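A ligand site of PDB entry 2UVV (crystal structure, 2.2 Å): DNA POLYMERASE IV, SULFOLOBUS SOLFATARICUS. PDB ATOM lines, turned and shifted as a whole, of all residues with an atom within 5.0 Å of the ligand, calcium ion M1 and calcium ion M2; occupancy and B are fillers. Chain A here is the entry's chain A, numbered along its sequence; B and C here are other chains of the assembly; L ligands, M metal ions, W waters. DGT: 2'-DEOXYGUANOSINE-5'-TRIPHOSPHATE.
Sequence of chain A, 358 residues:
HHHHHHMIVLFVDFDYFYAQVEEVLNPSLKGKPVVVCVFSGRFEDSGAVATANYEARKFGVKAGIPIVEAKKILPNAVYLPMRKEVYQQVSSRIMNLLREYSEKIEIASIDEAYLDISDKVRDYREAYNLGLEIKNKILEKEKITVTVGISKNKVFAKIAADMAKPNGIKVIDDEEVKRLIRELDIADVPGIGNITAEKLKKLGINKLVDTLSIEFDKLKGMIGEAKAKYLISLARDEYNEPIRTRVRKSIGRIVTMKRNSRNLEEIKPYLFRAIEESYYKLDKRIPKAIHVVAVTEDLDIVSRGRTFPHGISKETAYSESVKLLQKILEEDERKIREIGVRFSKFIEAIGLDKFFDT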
ATOM      1  N   ASP A  13       5.632 -27.529  -0.390  1.00  0.00           N
ATOM      2  CA  ASP A  13       6.759 -27.760  -1.284  1.00  0.00           C
ATOM      3  C   ASP A  13       6.197 -28.180  -2.652  1.00  0.00           C
ATOM      4  O   ASP A  13       5.591 -29.234  -2.768  1.00  0.00           O
ATOM      5  CB  ASP A  13       7.600 -28.883  -0.662  1.00  0.00           C
ATOM      6  CG  ASP A  13       8.949 -29.023  -1.311  1.00  0.00           C
ATOM      7  OD1 ASP A  13       9.837 -29.653  -0.734  1.00  0.00           O
ATOM      8  OD2 ASP A  13       9.116 -28.486  -2.414  1.00  0.00           O
ATOM      9  N   PHE A  14       6.406 -27.343  -3.679  1.00  0.00           N
ATOM     10  CA  PHE A  14       5.877 -27.596  -5.032  1.00  0.00           C
ATOM     11  C   PHE A  14       6.452 -28.855  -5.690  1.00  0.00           C
ATOM     12  O   PHE A  14       7.643 -29.074  -5.608  1.00  0.00           O
ATOM     13  CB  PHE A  14       6.152 -26.381  -5.936  1.00  0.00           C
ATOM     14  CG  PHE A  14       5.757 -25.041  -5.325  1.00  0.00           C
ATOM     15  CD1 PHE A  14       4.880 -24.977  -4.259  1.00  0.00           C
ATOM     16  CD2 PHE A  14       6.268 -23.855  -5.848  1.00  0.00           C
ATOM     17  CE1 PHE A  14       4.513 -23.738  -3.703  1.00  0.00           C
ATOM     18  CE2 PHE A  14       5.915 -22.619  -5.294  1.00  0.00           C
ATOM     19  CZ  PHE A  14       5.038 -22.554  -4.228  1.00  0.00           C
ATOM     20  N   ASP A  15       5.653 -29.686  -6.356  1.00  0.00           N
ATOM     21  CA  ASP A  15       6.232 -30.911  -6.933  1.00  0.00           C
ATOM     22  C   ASP A  15       7.065 -30.686  -8.211  1.00  0.00           C
ATOM     23  O   ASP A  15       6.653 -29.932  -9.096  1.00  0.00           O
ATOM     24  CB  ASP A  15       5.136 -31.962  -7.212  1.00  0.00           C
ATOM     25  CG  ASP A  15       4.289 -32.291  -5.973  1.00  0.00           C
ATOM     26  OD1 ASP A  15       4.794 -32.270  -4.835  1.00  0.00           O
ATOM     27  OD2 ASP A  15       3.087 -32.606  -6.161  1.00  0.00           O
ATOM     28  N   TYR A  16       8.219 -31.355  -8.293  1.00  0.00           N
ATOM     29  CA  TYR A  16       9.144 -31.254  -9.447  1.00  0.00           C
ATOM     30  C   TYR A  16       8.928 -29.935 -10.155  1.00  0.00           C
ATOM     31  O   TYR A  16       8.761 -29.866 -11.379  1.00  0.00           O
ATOM     32  CB  TYR A  16       8.962 -32.443 -10.405  1.00  0.00           C
ATOM     33  CG  TYR A  16       7.600 -32.605 -11.053  1.00  0.00           C
ATOM     34  CD1 TYR A  16       7.435 -32.399 -12.427  1.00  0.00           C
ATOM     35  CD2 TYR A  16       6.475 -32.956 -10.307  1.00  0.00           C
ATOM     36  CE1 TYR A  16       6.187 -32.535 -13.035  1.00  0.00           C
ATOM     37  CE2 TYR A  16       5.212 -33.089 -10.913  1.00  0.00           C
ATOM     38  CZ  TYR A  16       5.081 -32.873 -12.273  1.00  0.00           C
ATOM     39  OH  TYR A  16       3.847 -32.985 -12.868  1.00  0.00           O
ATOM     40  N   PHE A  17       8.978 -28.878  -9.357  1.00  0.00           N
ATOM     41  CA  PHE A  17       8.681 -27.533  -9.796  1.00  0.00           C
ATOM     42  C   PHE A  17       9.004 -27.037 -11.184  1.00  0.00           C
ATOM     43  O   PHE A  17       8.077 -26.788 -11.952  1.00  0.00           O
ATOM     44  CB  PHE A  17       9.143 -26.505  -8.769  1.00  0.00           C
ATOM     45  CG  PHE A  17       8.444 -25.175  -8.916  1.00  0.00           C
ATOM     46  CD1 PHE A  17       7.062 -25.129  -9.140  1.00  0.00           C
ATOM     47  CD2 PHE A  17       9.157 -23.980  -8.891  1.00  0.00           C
ATOM     48  CE1 PHE A  17       6.401 -23.925  -9.335  1.00  0.00           C
ATOM     49  CE2 PHE A  17       8.493 -22.753  -9.088  1.00  0.00           C
ATOM     50  CZ  PHE A  17       7.130 -22.724  -9.310  1.00  0.00           C
ATOM     51  N   TYR A  18      10.273 -26.874 -11.535  1.00  0.00           N
ATOM     52  CA  TYR A  18      10.597 -26.349 -12.859  1.00  0.00           C
ATOM     53  C   TYR A  18      10.026 -27.209 -13.996  1.00  0.00           C
ATOM     54  O   TYR A  18       9.567 -26.678 -15.012  1.00  0.00           O
ATOM     55  CB  TYR A  18      12.109 -26.241 -13.053  1.00  0.00           C
ATOM     56  CG  TYR A  18      12.855 -25.315 -12.133  1.00  0.00           C
ATOM     57  CD1 TYR A  18      12.208 -24.591 -11.117  1.00  0.00           C
ATOM     58  CD2 TYR A  18      14.226 -25.151 -12.273  1.00  0.00           C
ATOM     59  CE1 TYR A  18      12.930 -23.728 -10.268  1.00  0.00           C
ATOM     60  CE2 TYR A  18      14.956 -24.307 -11.444  1.00  0.00           C
ATOM     61  CZ  TYR A  18      14.317 -23.602 -10.448  1.00  0.00           C
ATOM     62  OH  TYR A  18      15.079 -22.792  -9.645  1.00  0.00           O
ATOM     63  N   VAL A  38      20.607 -27.125 -17.089  1.00  0.00           N
ATOM     64  CA  VAL A  38      21.393 -25.911 -17.044  1.00  0.00           C
ATOM     65  C   VAL A  38      22.615 -26.227 -17.901  1.00  0.00           C
ATOM     66  O   VAL A  38      23.546 -26.884 -17.443  1.00  0.00           O
ATOM     67  CB  VAL A  38      21.834 -25.580 -15.607  1.00  0.00           C
ATOM     68  CG1 VAL A  38      22.792 -24.379 -15.616  1.00  0.00           C
ATOM     69  CG2 VAL A  38      20.602 -25.255 -14.784  1.00  0.00           C
ATOM     70  N   VAL A  49      21.497 -31.311 -14.787  1.00  0.00           N
ATOM     71  CA  VAL A  49      20.043 -31.342 -14.724  1.00  0.00           C
ATOM     72  C   VAL A  49      19.588 -30.560 -13.476  1.00  0.00           C
ATOM     73  O   VAL A  49      20.010 -30.861 -12.358  1.00  0.00           O
ATOM     74  CB  VAL A  49      19.518 -32.797 -14.601  1.00  0.00           C
ATOM     75  CG1 VAL A  49      18.034 -32.777 -14.254  1.00  0.00           C
ATOM     76  CG2 VAL A  49      19.760 -33.554 -15.905  1.00  0.00           C
ATOM     77  N   ALA A  50      18.735 -29.561 -13.661  1.00  0.00           N
ATOM     78  CA  ALA A  50      18.215 -28.753 -12.554  1.00  0.00           C
ATOM     79  C   ALA A  50      17.192 -29.627 -11.848  1.00  0.00           C
ATOM     80  O   ALA A  50      17.174 -29.713 -10.619  1.00  0.00           O
ATOM     81  CB  ALA A  50      17.563 -27.469 -13.073  1.00  0.00           C
ATOM     82  N   THR A  51      16.331 -30.267 -12.638  1.00  0.00           N
ATOM     83  CA  THR A  51      15.320 -31.196 -12.129  1.00  0.00           C
ATOM     84  C   THR A  51      14.645 -31.980 -13.247  1.00  0.00           C
ATOM     85  O   THR A  51      14.827 -31.682 -14.431  1.00  0.00           O
ATOM     86  CB  THR A  51      14.232 -30.465 -11.300  1.00  0.00           C
ATOM     87  OG1 THR A  51      13.496 -31.437 -10.532  1.00  0.00           O
ATOM     88  CG2 THR A  51      13.262 -29.744 -12.199  1.00  0.00           C
ATOM     89  N   TYR A  54       8.648 -36.915 -12.552  1.00  0.00           N
ATOM     90  CA  TYR A  54       8.735 -38.265 -12.038  1.00  0.00           C
ATOM     91  C   TYR A  54       8.890 -39.360 -13.095  1.00  0.00           C
ATOM     92  O   TYR A  54       9.537 -40.376 -12.832  1.00  0.00           O
ATOM     93  CB  TYR A  54       7.578 -38.541 -11.060  1.00  0.00           C
ATOM     94  CG  TYR A  54       7.807 -37.827  -9.724  1.00  0.00           C
ATOM     95  CD1 TYR A  54       7.640 -36.438  -9.609  1.00  0.00           C
ATOM     96  CD2 TYR A  54       8.260 -38.521  -8.586  1.00  0.00           C
ATOM     97  CE1 TYR A  54       7.906 -35.767  -8.411  1.00  0.00           C
ATOM     98  CE2 TYR A  54       8.527 -37.853  -7.375  1.00  0.00           C
ATOM     99  CZ  TYR A  54       8.346 -36.473  -7.297  1.00  0.00           C
ATOM    100  OH  TYR A  54       8.598 -35.782  -6.122  1.00  0.00           O
ATOM    101  N   ARG A  57      12.574 -39.528 -13.369  1.00  0.00           N
ATOM    102  CA  ARG A  57      13.226 -40.004 -12.159  1.00  0.00           C
ATOM    103  C   ARG A  57      13.171 -41.517 -11.979  1.00  0.00           C
ATOM    104  O   ARG A  57      14.028 -42.103 -11.324  1.00  0.00           O
ATOM    105  CB  ARG A  57      12.636 -39.320 -10.931  1.00  0.00           C
ATOM    106  CG  ARG A  57      12.930 -37.839 -10.854  1.00  0.00           C
ATOM    107  CD  ARG A  57      12.376 -37.216  -9.585  1.00  0.00           C
ATOM    108  NE  ARG A  57      12.217 -35.776  -9.757  1.00  0.00           N
ATOM    109  CZ  ARG A  57      11.970 -34.914  -8.777  1.00  0.00           C
ATOM    110  NH1 ARG A  57      11.860 -35.352  -7.523  1.00  0.00           N
ATOM    111  NH2 ARG A  57      11.821 -33.621  -9.059  1.00  0.00           N
ATOM    112  N   ALA A  63      17.947 -34.291 -10.430  1.00  0.00           N
ATOM    113  CA  ALA A  63      18.709 -33.067 -10.264  1.00  0.00           C
ATOM    114  C   ALA A  63      20.143 -33.329  -9.884  1.00  0.00           C
ATOM    115  O   ALA A  63      20.418 -34.175  -9.046  1.00  0.00           O
ATOM    116  CB  ALA A  63      18.058 -32.195  -9.197  1.00  0.00           C
ATOM    117  N   GLY A  64      21.065 -32.595 -10.506  1.00  0.00           N
ATOM    118  CA  GLY A  64      22.465 -32.755 -10.165  1.00  0.00           C
ATOM    119  C   GLY A  64      23.309 -33.682 -11.014  1.00  0.00           C
ATOM    120  O   GLY A  64      24.534 -33.577 -11.003  1.00  0.00           O
ATOM    121  N   MET A  82      16.689 -24.399 -18.573  1.00  0.00           N
ATOM    122  CA  MET A  82      16.048 -23.756 -17.437  1.00  0.00           C
ATOM    123  C   MET A  82      15.668 -22.302 -17.749  1.00  0.00           C
ATOM    124  O   MET A  82      16.482 -21.535 -18.252  1.00  0.00           O
ATOM    125  CB  MET A  82      16.988 -23.816 -16.246  1.00  0.00           C
ATOM    126  CG  MET A  82      16.506 -23.075 -15.020  1.00  0.00           C
ATOM    127  SD  MET A  82      17.712 -23.167 -13.705  1.00  0.00           S
ATOM    128  CE  MET A  82      18.867 -21.896 -14.209  1.00  0.00           C
ATOM    129  N   SER A 109      12.257 -20.773  -0.210  1.00  0.00           N
ATOM    130  CA  SER A 109      12.947 -20.782  -1.503  1.00  0.00           C
ATOM    131  C   SER A 109      11.942 -20.593  -2.629  1.00  0.00           C
ATOM    132  O   SER A 109      10.769 -20.350  -2.363  1.00  0.00           O
ATOM    133  CB  SER A 109      13.705 -22.093  -1.707  1.00  0.00           C
ATOM    134  OG  SER A 109      12.816 -23.165  -1.986  1.00  0.00           O
ATOM    135  N   ILE A 110      12.401 -20.693  -3.866  1.00  0.00           N
ATOM    136  CA  ILE A 110      11.508 -20.519  -5.005  1.00  0.00           C
ATOM    137  C   ILE A 110      10.333 -21.519  -5.039  1.00  0.00           C
ATOM    138  O   ILE A 110       9.331 -21.275  -5.699  1.00  0.00           O
ATOM    139  CB  ILE A 110      12.297 -20.603  -6.361  1.00  0.00           C
ATOM    140  CG1 ILE A 110      11.371 -20.237  -7.523  1.00  0.00           C
ATOM    141  CG2 ILE A 110      12.870 -21.997  -6.547  1.00  0.00           C
ATOM    142  CD1 ILE A 110      12.109 -19.989  -8.839  1.00  0.00           C
ATOM    143  N   ASP A 111      10.417 -22.617  -4.318  1.00  0.00           N
ATOM    144  CA  ASP A 111       9.306 -23.557  -4.365  1.00  0.00           C
ATOM    145  C   ASP A 111       8.810 -24.072  -3.025  1.00  0.00           C
ATOM    146  O   ASP A 111       8.137 -25.087  -2.951  1.00  0.00           O
ATOM    147  CB  ASP A 111       9.672 -24.738  -5.227  1.00  0.00           C
ATOM    148  CG  ASP A 111      10.403 -25.791  -4.462  1.00  0.00           C
ATOM    149  OD1 ASP A 111      11.278 -25.455  -3.651  1.00  0.00           O
ATOM    150  OD2 ASP A 111      10.101 -26.950  -4.694  1.00  0.00           O
ATOM    151  N   GLU A 112       9.135 -23.358  -1.946  1.00  0.00           N
ATOM    152  CA  GLU A 112       8.693 -23.835  -0.652  1.00  0.00           C
ATOM    153  C   GLU A 112       8.457 -22.705   0.341  1.00  0.00           C
ATOM    154  O   GLU A 112       9.119 -21.662   0.296  1.00  0.00           O
ATOM    155  CB  GLU A 112       9.694 -24.859  -0.092  1.00  0.00           C
ATOM    156  CG  GLU A 112      10.980 -24.266   0.462  1.00  0.00           C
ATOM    157  CD  GLU A 112      11.968 -25.346   0.908  1.00  0.00           C
ATOM    158  OE1 GLU A 112      12.693 -25.139   1.905  1.00  0.00           O
ATOM    159  OE2 GLU A 112      12.021 -26.402   0.270  1.00  0.00           O
ATOM    160  N   LYS A 158       8.612 -29.905   7.466  1.00  0.00           N
ATOM    161  CA  LYS A 158       9.378 -30.187   6.268  1.00  0.00           C
ATOM    162  C   LYS A 158       9.630 -31.696   6.117  1.00  0.00           C
ATOM    163  O   LYS A 158       9.540 -32.235   5.024  1.00  0.00           O
ATOM    164  CB  LYS A 158      10.710 -29.459   6.297  1.00  0.00           C
ATOM    165  CG  LYS A 158      11.587 -29.769   5.098  1.00  0.00           C
ATOM    166  CD  LYS A 158      12.918 -29.057   5.203  1.00  0.00           C
ATOM    167  CE  LYS A 158      13.165 -28.199   3.988  1.00  0.00           C
ATOM    168  NZ  LYS A 158      13.174 -29.014   2.740  1.00  0.00           N
ATOM    169  N   LYS A 165       5.885 -36.747  -0.386  1.00  0.00           N
ATOM    170  CA  LYS A 165       6.098 -36.488  -1.816  1.00  0.00           C
ATOM    171  C   LYS A 165       5.788 -37.700  -2.710  1.00  0.00           C
ATOM    172  O   LYS A 165       6.135 -38.822  -2.382  1.00  0.00           O
ATOM    173  CB  LYS A 165       7.549 -36.034  -2.068  1.00  0.00           C
ATOM    174  CG  LYS A 165       7.868 -34.612  -1.613  1.00  0.00           C
ATOM    175  CD  LYS A 165       9.299 -34.182  -2.022  1.00  0.00           C
ATOM    176  CE  LYS A 165       9.600 -32.747  -1.555  1.00  0.00           C
ATOM    177  NZ  LYS A 165      10.955 -32.188  -1.986  1.00  0.00           N
ATOM    178  P    DC B   4      29.763 -28.726 -16.230  1.00  0.00           P
ATOM    179  OP1  DC B   4      28.915 -29.930 -16.581  1.00  0.00           O
ATOM    180  OP2  DC B   4      30.457 -28.119 -17.447  1.00  0.00           O
ATOM    181  O5'  DC B   4      28.735 -27.558 -15.731  1.00  0.00           O
ATOM    182  C5'  DC B   4      27.713 -27.843 -14.774  1.00  0.00           C
ATOM    183  C4'  DC B   4      26.644 -26.774 -14.836  1.00  0.00           C
ATOM    184  O4'  DC B   4      25.486 -27.182 -14.079  1.00  0.00           O
ATOM    185  C3'  DC B   4      27.152 -25.473 -14.192  1.00  0.00           C
ATOM    186  O3'  DC B   4      26.618 -24.354 -14.914  1.00  0.00           O
ATOM    187  C2'  DC B   4      26.584 -25.541 -12.789  1.00  0.00           C
ATOM    188  C1'  DC B   4      25.291 -26.334 -12.953  1.00  0.00           C
ATOM    189  N1   DC B   4      24.975 -27.201 -11.808  1.00  0.00           N
ATOM    190  C2   DC B   4      23.739 -27.048 -11.157  1.00  0.00           C
ATOM    191  O2   DC B   4      22.949 -26.186 -11.562  1.00  0.00           O
ATOM    192  N3   DC B   4      23.444 -27.857 -10.109  1.00  0.00           N
ATOM    193  C4   DC B   4      24.320 -28.781  -9.712  1.00  0.00           C
ATOM    194  N4   DC B   4      23.980 -29.552  -8.687  1.00  0.00           N
ATOM    195  C5   DC B   4      25.580 -28.963 -10.357  1.00  0.00           C
ATOM    196  C6   DC B   4      25.863 -28.154 -11.389  1.00  0.00           C
ATOM    197  P   8OG B   5      27.316 -22.905 -14.783  1.00  0.00           P
ATOM    198  OP1 8OG B   5      26.858 -22.119 -15.950  1.00  0.00           O
ATOM    199  OP2 8OG B   5      28.764 -23.042 -14.506  1.00  0.00           O
ATOM    200  O5' 8OG B   5      26.589 -22.238 -13.511  1.00  0.00           O
ATOM    201  C5' 8OG B   5      25.220 -21.836 -13.643  1.00  0.00           C
ATOM    202  C4' 8OG B   5      24.592 -21.625 -12.285  1.00  0.00           C
ATOM    203  O4' 8OG B   5      24.545 -22.891 -11.609  1.00  0.00           O
ATOM    204  C3' 8OG B   5      25.465 -20.720 -11.417  1.00  0.00           C
ATOM    205  O3' 8OG B   5      24.669 -19.913 -10.558  1.00  0.00           O
ATOM    206  C2' 8OG B   5      26.246 -21.729 -10.572  1.00  0.00           C
ATOM    207  C1' 8OG B   5      25.048 -22.634 -10.290  1.00  0.00           C
ATOM    208  N9  8OG B   5      25.339 -23.878  -9.534  1.00  0.00           N
ATOM    209  C8  8OG B   5      26.467 -24.580  -9.483  1.00  0.00           C
ATOM    210  N7  8OG B   5      26.356 -25.626  -8.675  1.00  0.00           N
ATOM    211  C5  8OG B   5      25.124 -25.588  -8.177  1.00  0.00           C
ATOM    212  C6  8OG B   5      24.434 -26.400  -7.279  1.00  0.00           C
ATOM    213  O6  8OG B   5      25.000 -27.375  -6.773  1.00  0.00           O
ATOM    214  N1  8OG B   5      23.111 -26.079  -6.953  1.00  0.00           N
ATOM    215  C2  8OG B   5      22.518 -24.956  -7.530  1.00  0.00           C
ATOM    216  N2  8OG B   5      21.272 -24.612  -7.205  1.00  0.00           N
ATOM    217  N3  8OG B   5      23.207 -24.191  -8.403  1.00  0.00           N
ATOM    218  C4  8OG B   5      24.473 -24.478  -8.723  1.00  0.00           C
ATOM    219  O8  8OG B   5      27.502 -24.320 -10.097  1.00  0.00           O
ATOM    220  P    DC C  14      16.266 -29.050  -0.087  1.00  0.00           P
ATOM    221  OP1  DC C  14      15.117 -29.281   0.821  1.00  0.00           O
ATOM    222  OP2  DC C  14      16.959 -30.201  -0.700  1.00  0.00           O
ATOM    223  O5'  DC C  14      15.840 -28.002  -1.237  1.00  0.00           O
ATOM    224  C5'  DC C  14      15.562 -26.653  -0.852  1.00  0.00           C
ATOM    225  C4'  DC C  14      15.736 -25.676  -1.995  1.00  0.00           C
ATOM    226  O4'  DC C  14      17.126 -25.581  -2.416  1.00  0.00           O
ATOM    227  C3'  DC C  14      14.932 -26.118  -3.224  1.00  0.00           C
ATOM    228  O3'  DC C  14      14.513 -24.957  -3.931  1.00  0.00           O
ATOM    229  C2'  DC C  14      16.007 -26.750  -4.101  1.00  0.00           C
ATOM    230  C1'  DC C  14      17.191 -25.860  -3.817  1.00  0.00           C
ATOM    231  N1   DC C  14      18.523 -26.422  -4.114  1.00  0.00           N
ATOM    232  C2   DC C  14      19.357 -25.739  -5.026  1.00  0.00           C
ATOM    233  O2   DC C  14      18.942 -24.676  -5.538  1.00  0.00           O
ATOM    234  N3   DC C  14      20.573 -26.260  -5.326  1.00  0.00           N
ATOM    235  C4   DC C  14      20.971 -27.394  -4.764  1.00  0.00           C
ATOM    236  N4   DC C  14      22.172 -27.860  -5.100  1.00  0.00           N
ATOM    237  C5   DC C  14      20.162 -28.108  -3.833  1.00  0.00           C
ATOM    238  C6   DC C  14      18.946 -27.587  -3.533  1.00  0.00           C
HETATM  239  PG  DGT L   1      10.387 -32.643  -5.784  1.00  0.00           P
HETATM  240  O1G DGT L   1       9.016 -33.026  -6.186  1.00  0.00           O
HETATM  241  O2G DGT L   1      10.367 -31.545  -4.606  1.00  0.00           O
HETATM  242  O3G DGT L   1      11.216 -33.876  -5.173  1.00  0.00           O
HETATM  243  O3B DGT L   1      11.289 -32.089  -7.003  1.00  0.00           O
HETATM  244  PB  DGT L   1      11.801 -30.571  -7.161  1.00  0.00           P
HETATM  245  O1B DGT L   1      10.750 -29.640  -6.710  1.00  0.00           O
HETATM  246  O2B DGT L   1      12.254 -30.431  -8.566  1.00  0.00           O
HETATM  247  O3A DGT L   1      13.113 -30.541  -6.234  1.00  0.00           O
HETATM  248  PA  DGT L   1      13.375 -29.692  -4.883  1.00  0.00           P
HETATM  249  O1A DGT L   1      12.081 -28.969  -4.259  1.00  0.00           O
HETATM  250  O2A DGT L   1      14.580 -29.936  -4.072  1.00  0.00           O
HETATM  251  O5' DGT L   1      13.899 -28.388  -5.663  1.00  0.00           O
HETATM  252  C5' DGT L   1      13.023 -27.367  -6.162  1.00  0.00           C
HETATM  253  C4' DGT L   1      13.614 -26.688  -7.397  1.00  0.00           C
HETATM  254  O4' DGT L   1      14.935 -26.174  -7.150  1.00  0.00           O
HETATM  255  C3' DGT L   1      13.806 -27.703  -8.526  1.00  0.00           C
HETATM  256  O3' DGT L   1      12.568 -27.864  -9.229  1.00  0.00           O
HETATM  257  C2' DGT L   1      14.767 -26.903  -9.399  1.00  0.00           C
HETATM  258  C1' DGT L   1      15.726 -26.349  -8.338  1.00  0.00           C
HETATM  259  N9  DGT L   1      16.834 -27.287  -8.050  1.00  0.00           N
HETATM  260  C8  DGT L   1      16.812 -28.296  -7.182  1.00  0.00           C
HETATM  261  N7  DGT L   1      18.001 -28.899  -7.171  1.00  0.00           N
HETATM  262  C5  DGT L   1      18.790 -28.277  -8.043  1.00  0.00           C
HETATM  263  C6  DGT L   1      20.112 -28.464  -8.446  1.00  0.00           C
HETATM  264  O6  DGT L   1      20.809 -29.346  -7.936  1.00  0.00           O
HETATM  265  N1  DGT L   1      20.655 -27.611  -9.409  1.00  0.00           N
HETATM  266  C2  DGT L   1      19.863 -26.583  -9.942  1.00  0.00           C
HETATM  267  N2  DGT L   1      20.371 -25.737 -10.831  1.00  0.00           N
HETATM  268  N3  DGT L   1      18.594 -26.434  -9.523  1.00  0.00           N
HETATM  269  C4  DGT L   1      18.047 -27.246  -8.601  1.00  0.00           C
HETATM  270 CA    CA M   1      11.955 -27.751  -1.918  1.00  0.00          CA
HETATM  271 CA    CA M   2       9.773 -29.308  -4.630  1.00  0.00          CA
HETATM  272  O   HOH W   1      21.431 -31.366  -6.679  1.00  0.00           O
HETATM  273  O   HOH W   2      12.588 -29.388  -0.687  1.00  0.00           O
HETATM  274  O   HOH W   3       7.359 -31.578  -3.342  1.00  0.00           O
HETATM  275  O   HOH W   4      10.546 -36.950  -4.187  1.00  0.00           O
HETATM  276  O   HOH W   5      17.803 -23.246  -9.463  1.00  0.00           O
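An oxygen (O2B) of the ligand is in hydrogen-bond range of the side-chain hydroxyl (OG1) of Thr 51 (2.5 Å).
NH1 of Arg 57 lies within salt-bridge range of O3G of the ligand, 2.8 Å away.
A nitrogen (N2) of the ligand lies within hydrogen-bond range of O2 of DC 4 of chain B (2.7 Å).
NZ of Lys 165 is in salt-bridge range of O3G of the ligand, at 3.6 Å.
An oxygen (O1G) of the ligand lies within hydrogen-bond range of the side-chain hydroxyl of Tyr 54, 2.8 Å away.
N of Tyr 16 lies within hydrogen-bond range of O1G of the ligand (2.8 Å).
O1B of the ligand lies close to N of Phe 17 (3.3 Å).
The backbone NH (N) of Tyr 18 lies within hydrogen-bond range of an oxygen (O3') of the ligand, 3.4 Å away.
The side-chain carboxylate (OD1) of Asp 111 is in hydrogen-bond range of the side-chain hydroxyl (OG) of Ser 109 (3.2 Å).
The side-chain carboxylate (OD1) of Asp 13 is in salt-bridge range of the side-chain amino group (NZ) of Lys 165, at 3.0 Å.
The side-chain hydroxyl (OG1) of Thr 51 sits at hydrogen-bond distance from the guanidinium group (NH2) of Arg 57.
The side-chain amino group of Lys 158 is in salt-bridge range of the side-chain carboxylate of Glu 112.
N3 of DC 14 of chain C lies close to N2 of 8OG 5 of chain B.
The side-chain hydroxyl of Ser 109 lies within hydrogen-bond range of O3' of DC 14 of chain C (3.1 Å).
The side-chain amino group (NZ) of Lys 158 lies within salt-bridge range of OP1 of DC 14 of chain C, at 2.7 Å.
O3' of DC 14 of chain C lies close to an oxygen (O4') of the ligand, at 3.5 Å.
Asp 15 touches the ligand (CA to O1G, 3.6 Å).
CG2 of Val 38 touches N2 of the ligand, 3.99 Å away.
Ala 50 touches the ligand.
Ala 63 touches the ligand.
8OG 5 of chain B touches the ligand (N2 to C2, 3.7 Å).
Hydrophobic or aromatic side chains within 4 Å of the ligand: Phe 17, Tyr 18, Val 38, Ala 50, Tyr 54 and Ala 63.
Merely in contact with calcium ion M1: DC 14 of chain C (3.6 Å).
Within 4 Å of calcium ion M1: Asp 13, Asp 111, Glu 112 and DC 14 of chain C.
The nearest printed residue that does not touch calcium ion M1 is Lys 165 (4.5 Å).
Three residues have an atom within 4 Å of calcium ion M2: Asp 13, Phe 14 of chain A and Asp 111.
The nearest printed residue that does not touch calcium ion M2 is Lys 165 (4.1 Å).
Calcium ion M1 is bound by water W2 (2.1 Å).
OE2 of Glu 112 is bound to calcium ion M1 (2.6 Å).
Calcium ion M1 is bound by an oxygen (O1A) of the ligand (2.6 Å).
Slightly farther from calcium ion M1 lies OD1 of Asp 111 (3.0 Å).
Slightly farther from calcium ion M1 lies the side-chain carboxylate (OD2) of Asp 13 (3.0 Å).
Slightly farther from calcium ion M1 lies the side-chain carboxylate (OD1) of Asp 13 (3.1 Å).
Calcium ion M2 is bound by an oxygen (O2G) of the ligand, an oxygen (O1B) of the ligand, the backbone carbonyl oxygen (O) of Phe 14 of chain A, an oxygen (O1A) of the ligand, the side-chain carboxylate (OD2) of Asp 111 and the side-chain carboxylate (OD2) of Asp 13.
Calcium ion M2 has six donor atoms within binding distance.
Water W2 lies within hydrogen-bond range of OD1 of Asp 13 (2.8 Å), OP1 of DC 14 of chain C (2.9 Å), NZ of Lys 165 (3.5 Å) and NZ of Lys 158 (3.5 Å).
Water W3 bridges O of Asp 13 (3.0 Å) and OD1 of Asp 15 (3.0 Å).
Water W5 lies within hydrogen-bond range of OH of Tyr 18 and N3 of the ligand.
Water W4 lies within hydrogen-bond range of OH of Tyr 54 and O3G of the ligand.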
